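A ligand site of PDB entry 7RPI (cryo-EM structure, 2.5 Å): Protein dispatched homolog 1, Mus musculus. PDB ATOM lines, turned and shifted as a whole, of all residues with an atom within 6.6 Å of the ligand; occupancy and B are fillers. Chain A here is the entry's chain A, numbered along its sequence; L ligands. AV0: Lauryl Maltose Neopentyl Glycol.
OD1 of Asp 333 sits at hydrogen-bond distance from OAI of the ligand.
An oxygen (OAQ) of the ligand sits at hydrogen-bond distance from the side-chain hydroxyl of Tyr 336, 2.8 Å away.
OD2 of Asp 333 sits at hydrogen-bond distance from N of Thr 930 (2.8 Å).
The side-chain carboxylate of Asp 333 lies within hydrogen-bond range of the side-chain hydroxyl of Ser 929.
The backbone carbonyl oxygen of Pro 928 sits at hydrogen-bond distance from the side-chain hydroxyl of Tyr 336, 3.0 Å away.
The side-chain hydroxyl (OG1) of Thr 334 sits at hydrogen-bond distance from the backbone carbonyl oxygen (O) of Leu 331 (2.7 Å).
Met 332 touches the ligand (O to CBM, 3.4 Å).
Thr 334 touches the ligand (O to CBF, 3.7 Å).
CG1 of Val 335 touches OAQ of the ligand (3.6 Å).
CB of Ala 338 touches CBB of the ligand, 3.8 Å away.
Ile 366 touches the ligand.
Leu 393 touches the ligand.
Of the 19 residues printed, 8 come within 4 Å of the ligand.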
ATOM      1  N   ASP A 328      14.637  18.771  15.319  1.00  0.00           N
ATOM      2  CA  ASP A 328      14.968  19.628  14.183  1.00  0.00           C
ATOM      3  C   ASP A 328      14.375  21.021  14.341  1.00  0.00           C
ATOM      4  O   ASP A 328      15.101  22.010  14.289  1.00  0.00           O
ATOM      5  CB  ASP A 328      14.493  18.975  12.873  1.00  0.00           C
ATOM      6  CG  ASP A 328      15.173  17.641  12.561  1.00  0.00           C
ATOM      7  OD1 ASP A 328      16.244  17.341  13.151  1.00  0.00           O
ATOM      8  OD2 ASP A 328      14.691  16.919  11.665  1.00  0.00           O
ATOM      9  N   TYR A 329      13.083  21.120  14.629  1.00  0.00           N
ATOM     10  CA  TYR A 329      12.430  22.412  14.882  1.00  0.00           C
ATOM     11  C   TYR A 329      12.953  23.102  16.138  1.00  0.00           C
ATOM     12  O   TYR A 329      13.116  24.315  16.146  1.00  0.00           O
ATOM     13  CB  TYR A 329      10.922  22.208  14.955  1.00  0.00           C
ATOM     14  CG  TYR A 329      10.219  21.753  13.687  1.00  0.00           C
ATOM     15  CD1 TYR A 329      10.887  21.694  12.439  1.00  0.00           C
ATOM     16  CD2 TYR A 329       8.857  21.445  13.744  1.00  0.00           C
ATOM     17  CE1 TYR A 329      10.187  21.333  11.279  1.00  0.00           C
ATOM     18  CE2 TYR A 329       8.149  21.089  12.582  1.00  0.00           C
ATOM     19  CZ  TYR A 329       8.809  21.043  11.344  1.00  0.00           C
ATOM     20  OH  TYR A 329       8.126  20.708  10.224  1.00  0.00           O
ATOM     21  N   LEU A 331      16.027  23.131  17.346  1.00  0.00           N
ATOM     22  CA  LEU A 331      17.252  23.825  16.960  1.00  0.00           C
ATOM     23  C   LEU A 331      17.014  24.875  15.879  1.00  0.00           C
ATOM     24  O   LEU A 331      17.536  25.978  15.995  1.00  0.00           O
ATOM     25  CB  LEU A 331      18.322  22.807  16.551  1.00  0.00           C
ATOM     26  CG  LEU A 331      18.736  21.830  17.668  1.00  0.00           C
ATOM     27  CD1 LEU A 331      19.870  20.937  17.158  1.00  0.00           C
ATOM     28  CD2 LEU A 331      19.205  22.534  18.929  1.00  0.00           C
ATOM     29  N   MET A 332      16.221  24.594  14.846  1.00  0.00           N
ATOM     30  CA  MET A 332      15.928  25.583  13.793  1.00  0.00           C
ATOM     31  C   MET A 332      15.313  26.873  14.345  1.00  0.00           C
ATOM     32  O   MET A 332      15.701  27.961  13.947  1.00  0.00           O
ATOM     33  CB  MET A 332      14.965  24.994  12.761  1.00  0.00           C
ATOM     34  CG  MET A 332      15.583  23.956  11.816  1.00  0.00           C
ATOM     35  SD  MET A 332      14.375  23.021  10.852  1.00  0.00           S
ATOM     36  CE  MET A 332      13.574  24.352   9.912  1.00  0.00           C
ATOM     37  N   ASP A 333      14.391  26.773  15.307  1.00  0.00           N
ATOM     38  CA  ASP A 333      13.742  27.927  15.906  1.00  0.00           C
ATOM     39  C   ASP A 333      14.657  28.777  16.803  1.00  0.00           C
ATOM     40  O   ASP A 333      14.253  29.858  17.221  1.00  0.00           O
ATOM     41  CB  ASP A 333      12.475  27.493  16.670  1.00  0.00           C
ATOM     42  CG  ASP A 333      11.276  27.171  15.771  1.00  0.00           C
ATOM     43  OD1 ASP A 333      11.431  27.138  14.535  1.00  0.00           O
ATOM     44  OD2 ASP A 333      10.147  27.071  16.303  1.00  0.00           O
ATOM     45  N   THR A 334      15.910  28.390  17.052  1.00  0.00           N
ATOM     46  CA  THR A 334      16.887  29.277  17.709  1.00  0.00           C
ATOM     47  C   THR A 334      17.254  30.516  16.876  1.00  0.00           C
ATOM     48  O   THR A 334      17.864  31.445  17.394  1.00  0.00           O
ATOM     49  CB  THR A 334      18.166  28.555  18.150  1.00  0.00           C
ATOM     50  OG1 THR A 334      18.850  28.027  17.053  1.00  0.00           O
ATOM     51  CG2 THR A 334      17.890  27.422  19.143  1.00  0.00           C
ATOM     52  N   VAL A 335      16.777  30.598  15.632  1.00  0.00           N
ATOM     53  CA  VAL A 335      16.796  31.836  14.851  1.00  0.00           C
ATOM     54  C   VAL A 335      15.984  32.970  15.487  1.00  0.00           C
ATOM     55  O   VAL A 335      16.372  34.127  15.374  1.00  0.00           O
ATOM     56  CB  VAL A 335      16.351  31.534  13.401  1.00  0.00           C
ATOM     57  CG1 VAL A 335      14.862  31.244  13.259  1.00  0.00           C
ATOM     58  CG2 VAL A 335      16.740  32.685  12.470  1.00  0.00           C
ATOM     59  N   TYR A 336      14.893  32.700  16.214  1.00  0.00           N
ATOM     60  CA  TYR A 336      14.068  33.772  16.807  1.00  0.00           C
ATOM     61  C   TYR A 336      14.708  34.498  18.012  1.00  0.00           C
ATOM     62  O   TYR A 336      14.699  35.719  18.016  1.00  0.00           O
ATOM     63  CB  TYR A 336      12.660  33.262  17.122  1.00  0.00           C
ATOM     64  CG  TYR A 336      11.938  32.636  15.954  1.00  0.00           C
ATOM     65  CD1 TYR A 336      11.679  33.393  14.800  1.00  0.00           C
ATOM     66  CD2 TYR A 336      11.543  31.279  16.010  1.00  0.00           C
ATOM     67  CE1 TYR A 336      11.021  32.807  13.702  1.00  0.00           C
ATOM     68  CE2 TYR A 336      10.864  30.702  14.917  1.00  0.00           C
ATOM     69  CZ  TYR A 336      10.599  31.472  13.772  1.00  0.00           C
ATOM     70  OH  TYR A 336       9.879  30.940  12.755  1.00  0.00           O
ATOM     71  N   PRO A 337      15.331  33.815  18.989  1.00  0.00           N
ATOM     72  CA  PRO A 337      16.191  34.448  19.970  1.00  0.00           C
ATOM     73  C   PRO A 337      17.385  35.203  19.389  1.00  0.00           C
ATOM     74  O   PRO A 337      17.798  36.176  19.984  1.00  0.00           O
ATOM     75  CB  PRO A 337      16.679  33.342  20.884  1.00  0.00           C
ATOM     76  CG  PRO A 337      15.731  32.211  20.653  1.00  0.00           C
ATOM     77  CD  PRO A 337      15.232  32.408  19.256  1.00  0.00           C
ATOM     78  N   ALA A 338      17.933  34.804  18.242  1.00  0.00           N
ATOM     79  CA  ALA A 338      18.982  35.519  17.533  1.00  0.00           C
ATOM     80  C   ALA A 338      18.478  36.842  16.937  1.00  0.00           C
ATOM     81  O   ALA A 338      19.121  37.877  17.075  1.00  0.00           O
ATOM     82  CB  ALA A 338      19.565  34.591  16.472  1.00  0.00           C
ATOM     83  N   ILE A 339      17.283  36.869  16.347  1.00  0.00           N
ATOM     84  CA  ILE A 339      16.643  38.112  15.908  1.00  0.00           C
ATOM     85  C   ILE A 339      16.350  39.012  17.116  1.00  0.00           C
ATOM     86  O   ILE A 339      16.583  40.211  17.051  1.00  0.00           O
ATOM     87  CB  ILE A 339      15.395  37.790  15.056  1.00  0.00           C
ATOM     88  CG1 ILE A 339      15.771  37.049  13.757  1.00  0.00           C
ATOM     89  CG2 ILE A 339      14.632  39.083  14.698  1.00  0.00           C
ATOM     90  CD1 ILE A 339      14.604  36.251  13.162  1.00  0.00           C
ATOM     91  N   ILE A 341      18.132  39.292  19.926  1.00  0.00           N
ATOM     92  CA  ILE A 341      19.449  39.867  20.226  1.00  0.00           C
ATOM     93  C   ILE A 341      19.709  41.124  19.433  1.00  0.00           C
ATOM     94  O   ILE A 341      20.078  42.106  20.035  1.00  0.00           O
ATOM     95  CB  ILE A 341      20.576  38.832  20.015  1.00  0.00           C
ATOM     96  CG1 ILE A 341      20.572  37.821  21.146  1.00  0.00           C
ATOM     97  CG2 ILE A 341      21.975  39.440  19.857  1.00  0.00           C
ATOM     98  CD1 ILE A 341      21.381  36.568  20.887  1.00  0.00           C
ATOM     99  N   ILE A 366      25.712  36.610  26.428  1.00  0.00           N
ATOM    100  CA  ILE A 366      25.944  35.311  25.820  1.00  0.00           C
ATOM    101  C   ILE A 366      26.997  34.517  26.547  1.00  0.00           C
ATOM    102  O   ILE A 366      26.832  33.343  26.766  1.00  0.00           O
ATOM    103  CB  ILE A 366      26.176  35.468  24.314  1.00  0.00           C
ATOM    104  CG1 ILE A 366      25.049  36.234  23.579  1.00  0.00           C
ATOM    105  CG2 ILE A 366      26.378  34.096  23.656  1.00  0.00           C
ATOM    106  CD1 ILE A 366      23.641  35.760  23.888  1.00  0.00           C
ATOM    107  N   LEU A 369      25.606  32.336  29.547  1.00  0.00           N
ATOM    108  CA  LEU A 369      25.048  31.051  29.121  1.00  0.00           C
ATOM    109  C   LEU A 369      26.117  29.977  28.949  1.00  0.00           C
ATOM    110  O   LEU A 369      25.935  28.859  29.403  1.00  0.00           O
ATOM    111  CB  LEU A 369      24.260  31.227  27.825  1.00  0.00           C
ATOM    112  CG  LEU A 369      22.973  32.038  28.009  1.00  0.00           C
ATOM    113  CD1 LEU A 369      22.431  32.523  26.695  1.00  0.00           C
ATOM    114  CD2 LEU A 369      21.875  31.265  28.726  1.00  0.00           C
ATOM    115  N   LEU A 390      17.124  25.108  26.690  1.00  0.00           N
ATOM    116  CA  LEU A 390      17.234  25.982  25.525  1.00  0.00           C
ATOM    117  C   LEU A 390      16.404  27.261  25.653  1.00  0.00           C
ATOM    118  O   LEU A 390      16.754  28.282  25.075  1.00  0.00           O
ATOM    119  CB  LEU A 390      16.821  25.214  24.265  1.00  0.00           C
ATOM    120  CG  LEU A 390      17.878  24.216  23.769  1.00  0.00           C
ATOM    121  CD1 LEU A 390      17.224  23.275  22.768  1.00  0.00           C
ATOM    122  CD2 LEU A 390      19.039  24.919  23.065  1.00  0.00           C
ATOM    123  N   LEU A 393      18.113  30.795  26.851  1.00  0.00           N
ATOM    124  CA  LEU A 393      18.517  31.789  25.874  1.00  0.00           C
ATOM    125  C   LEU A 393      17.437  32.861  25.637  1.00  0.00           C
ATOM    126  O   LEU A 393      17.775  34.011  25.474  1.00  0.00           O
ATOM    127  CB  LEU A 393      18.904  31.021  24.606  1.00  0.00           C
ATOM    128  CG  LEU A 393      19.329  31.864  23.395  1.00  0.00           C
ATOM    129  CD1 LEU A 393      20.616  32.637  23.623  1.00  0.00           C
ATOM    130  CD2 LEU A 393      19.515  30.917  22.219  1.00  0.00           C
ATOM    131  N   PRO A 928       6.389  33.427  16.145  1.00  0.00           N
ATOM    132  CA  PRO A 928       6.467  32.588  14.945  1.00  0.00           C
ATOM    133  C   PRO A 928       6.993  31.147  15.153  1.00  0.00           C
ATOM    134  O   PRO A 928       7.233  30.448  14.184  1.00  0.00           O
ATOM    135  CB  PRO A 928       7.333  33.372  13.961  1.00  0.00           C
ATOM    136  CG  PRO A 928       8.184  34.270  14.843  1.00  0.00           C
ATOM    137  CD  PRO A 928       7.251  34.584  15.999  1.00  0.00           C
ATOM    138  N   SER A 929       7.224  30.704  16.388  1.00  0.00           N
ATOM    139  CA  SER A 929       7.823  29.393  16.657  1.00  0.00           C
ATOM    140  C   SER A 929       6.859  28.219  16.522  1.00  0.00           C
ATOM    141  O   SER A 929       5.697  28.303  16.916  1.00  0.00           O
ATOM    142  CB  SER A 929       8.485  29.422  18.030  1.00  0.00           C
ATOM    143  OG  SER A 929       9.032  28.176  18.363  1.00  0.00           O
ATOM    144  N   THR A 930       7.346  27.082  16.030  1.00  0.00           N
ATOM    145  CA  THR A 930       6.581  25.824  15.994  1.00  0.00           C
ATOM    146  C   THR A 930       6.625  25.110  17.336  1.00  0.00           C
ATOM    147  O   THR A 930       5.677  24.410  17.698  1.00  0.00           O
ATOM    148  CB  THR A 930       7.127  24.894  14.889  1.00  0.00           C
ATOM    149  OG1 THR A 930       7.107  25.561  13.666  1.00  0.00           O
ATOM    150  CG2 THR A 930       6.280  23.644  14.688  1.00  0.00           C
HETATM  151  C1  AV0 L   1      18.215  27.071   8.454  1.00  0.00           C
HETATM  152  O1  AV0 L   1      17.862  27.028   9.859  1.00  0.00           O
HETATM  153  C2  AV0 L   1      17.269  26.137   7.621  1.00  0.00           C
HETATM  154  O2  AV0 L   1      17.928  25.602   6.473  1.00  0.00           O
HETATM  155  C3  AV0 L   1      15.983  26.895   7.151  1.00  0.00           C
HETATM  156  O3  AV0 L   1      14.938  25.941   6.919  1.00  0.00           O
HETATM  157  C4  AV0 L   1      15.604  27.994   8.184  1.00  0.00           C
HETATM  158  O4  AV0 L   1      14.389  28.711   7.849  1.00  0.00           O
HETATM  159  C5  AV0 L   1      16.751  29.039   8.238  1.00  0.00           C
HETATM  160  O5  AV0 L   1      18.050  28.432   8.008  1.00  0.00           O
HETATM  161  C6  AV0 L   1      16.727  29.840   9.557  1.00  0.00           C
HETATM  162  O6  AV0 L   1      15.657  30.779   9.478  1.00  0.00           O
HETATM  163  CAA AV0 L   1      23.004  28.706  22.027  1.00  0.00           C
HETATM  164  CAB AV0 L   1      23.595  32.516  21.288  1.00  0.00           C
HETATM  165  OAI AV0 L   1      11.982  27.298  12.063  1.00  0.00           O
HETATM  166  OAJ AV0 L   1      24.478  33.290   4.157  1.00  0.00           O
HETATM  167  OAL AV0 L   1      24.592  31.705   6.576  1.00  0.00           O
HETATM  168  OAN AV0 L   1      22.502  26.792   4.884  1.00  0.00           O
HETATM  169  OAP AV0 L   1      21.543  25.804   7.374  1.00  0.00           O
HETATM  170  OAQ AV0 L   1      12.058  30.924  11.023  1.00  0.00           O
HETATM  171  OAR AV0 L   1      27.700  30.880   2.608  1.00  0.00           O
HETATM  172  OAS AV0 L   1      10.782  30.997   8.383  1.00  0.00           O
HETATM  173  OAT AV0 L   1      27.146  28.126   1.924  1.00  0.00           O
HETATM  174  OAU AV0 L   1      12.048  29.390   6.388  1.00  0.00           O
HETATM  175  OAV AV0 L   1      24.827  26.951   3.254  1.00  0.00           O
HETATM  176  CAW AV0 L   1      22.229  27.705  21.168  1.00  0.00           C
HETATM  177  CAX AV0 L   1      22.656  32.764  20.088  1.00  0.00           C
HETATM  178  CAY AV0 L   1      23.133  27.124  20.066  1.00  0.00           C
HETATM  179  CAZ AV0 L   1      22.449  31.495  19.230  1.00  0.00           C
HETATM  180  CBA AV0 L   1      22.385  26.184  19.107  1.00  0.00           C
HETATM  181  CBB AV0 L   1      21.631  31.817  17.963  1.00  0.00           C
HETATM  182  CBC AV0 L   1      23.359  25.555  18.086  1.00  0.00           C
HETATM  183  CBD AV0 L   1      21.642  30.660  16.937  1.00  0.00           C
HETATM  184  CBE AV0 L   1      22.637  24.833  16.929  1.00  0.00           C
HETATM  185  CBF AV0 L   1      21.030  31.088  15.582  1.00  0.00           C
HETATM  186  CBG AV0 L   1      22.324  25.833  15.796  1.00  0.00           C
HETATM  187  CBH AV0 L   1      20.989  29.916  14.579  1.00  0.00           C
HETATM  188  CBI AV0 L   1      21.503  25.199  14.669  1.00  0.00           C
HETATM  189  CBJ AV0 L   1      20.472  30.351  13.193  1.00  0.00           C
HETATM  190  CBK AV0 L   1      21.305  26.232  13.536  1.00  0.00           C
HETATM  191  CBL AV0 L   1      20.674  29.252  12.111  1.00  0.00           C
HETATM  192  CBM AV0 L   1      13.031  28.245  11.913  1.00  0.00           C
HETATM  193  CBN AV0 L   1      25.312  32.663   3.174  1.00  0.00           C
HETATM  194  CBP AV0 L   1      23.352  31.247   7.134  1.00  0.00           C
HETATM  195  CBQ AV0 L   1      20.215  25.790  12.543  1.00  0.00           C
HETATM  196  CBR AV0 L   1      19.505  28.223  11.999  1.00  0.00           C
HETATM  197  CBS AV0 L   1      18.627  26.124  10.667  1.00  0.00           C
HETATM  198  CBT AV0 L   1      21.094  26.858  10.396  1.00  0.00           C
HETATM  199  OBV AV0 L   1      20.928  27.890   9.412  1.00  0.00           O
HETATM  200  OBX AV0 L   1      22.175  29.397   8.142  1.00  0.00           O
HETATM  201  OBY AV0 L   1      13.070  27.698   9.536  1.00  0.00           O
HETATM  202  OBZ AV0 L   1      24.050  30.593   3.214  1.00  0.00           O
HETATM  203  OCB AV0 L   1      24.183  29.137   5.039  1.00  0.00           O
HETATM  204  CCC AV0 L   1      13.099  28.802  10.474  1.00  0.00           C
HETATM  205  CCD AV0 L   1      25.377  31.136   3.407  1.00  0.00           C
HETATM  206  CCF AV0 L   1      23.288  29.699   7.268  1.00  0.00           C
HETATM  207  CCH AV0 L   1      22.805  27.462   6.117  1.00  0.00           C
HETATM  208  CCJ AV0 L   1      22.020  28.003   8.466  1.00  0.00           C
HETATM  209  CCL AV0 L   1      21.684  27.222   7.155  1.00  0.00           C
HETATM  210  CCM AV0 L   1      19.871  26.802  11.379  1.00  0.00           C
HETATM  211  CCN AV0 L   1      11.927  29.774  10.184  1.00  0.00           C
HETATM  212  CCO AV0 L   1      26.358  30.375   2.468  1.00  0.00           C
HETATM  213  CCQ AV0 L   1      23.033  28.987   5.897  1.00  0.00           C
HETATM  214  CCR AV0 L   1      13.149  28.022   8.125  1.00  0.00           C
HETATM  215  CCS AV0 L   1      23.895  29.220   3.625  1.00  0.00           C
HETATM  216  CCT AV0 L   1      11.936  30.204   8.688  1.00  0.00           C
HETATM  217  CCU AV0 L   1      26.322  28.860   2.838  1.00  0.00           C
HETATM  218  CCV AV0 L   1      11.968  28.964   7.754  1.00  0.00           C
HETATM  219  CCW AV0 L   1      24.867  28.313   2.803  1.00  0.00           C
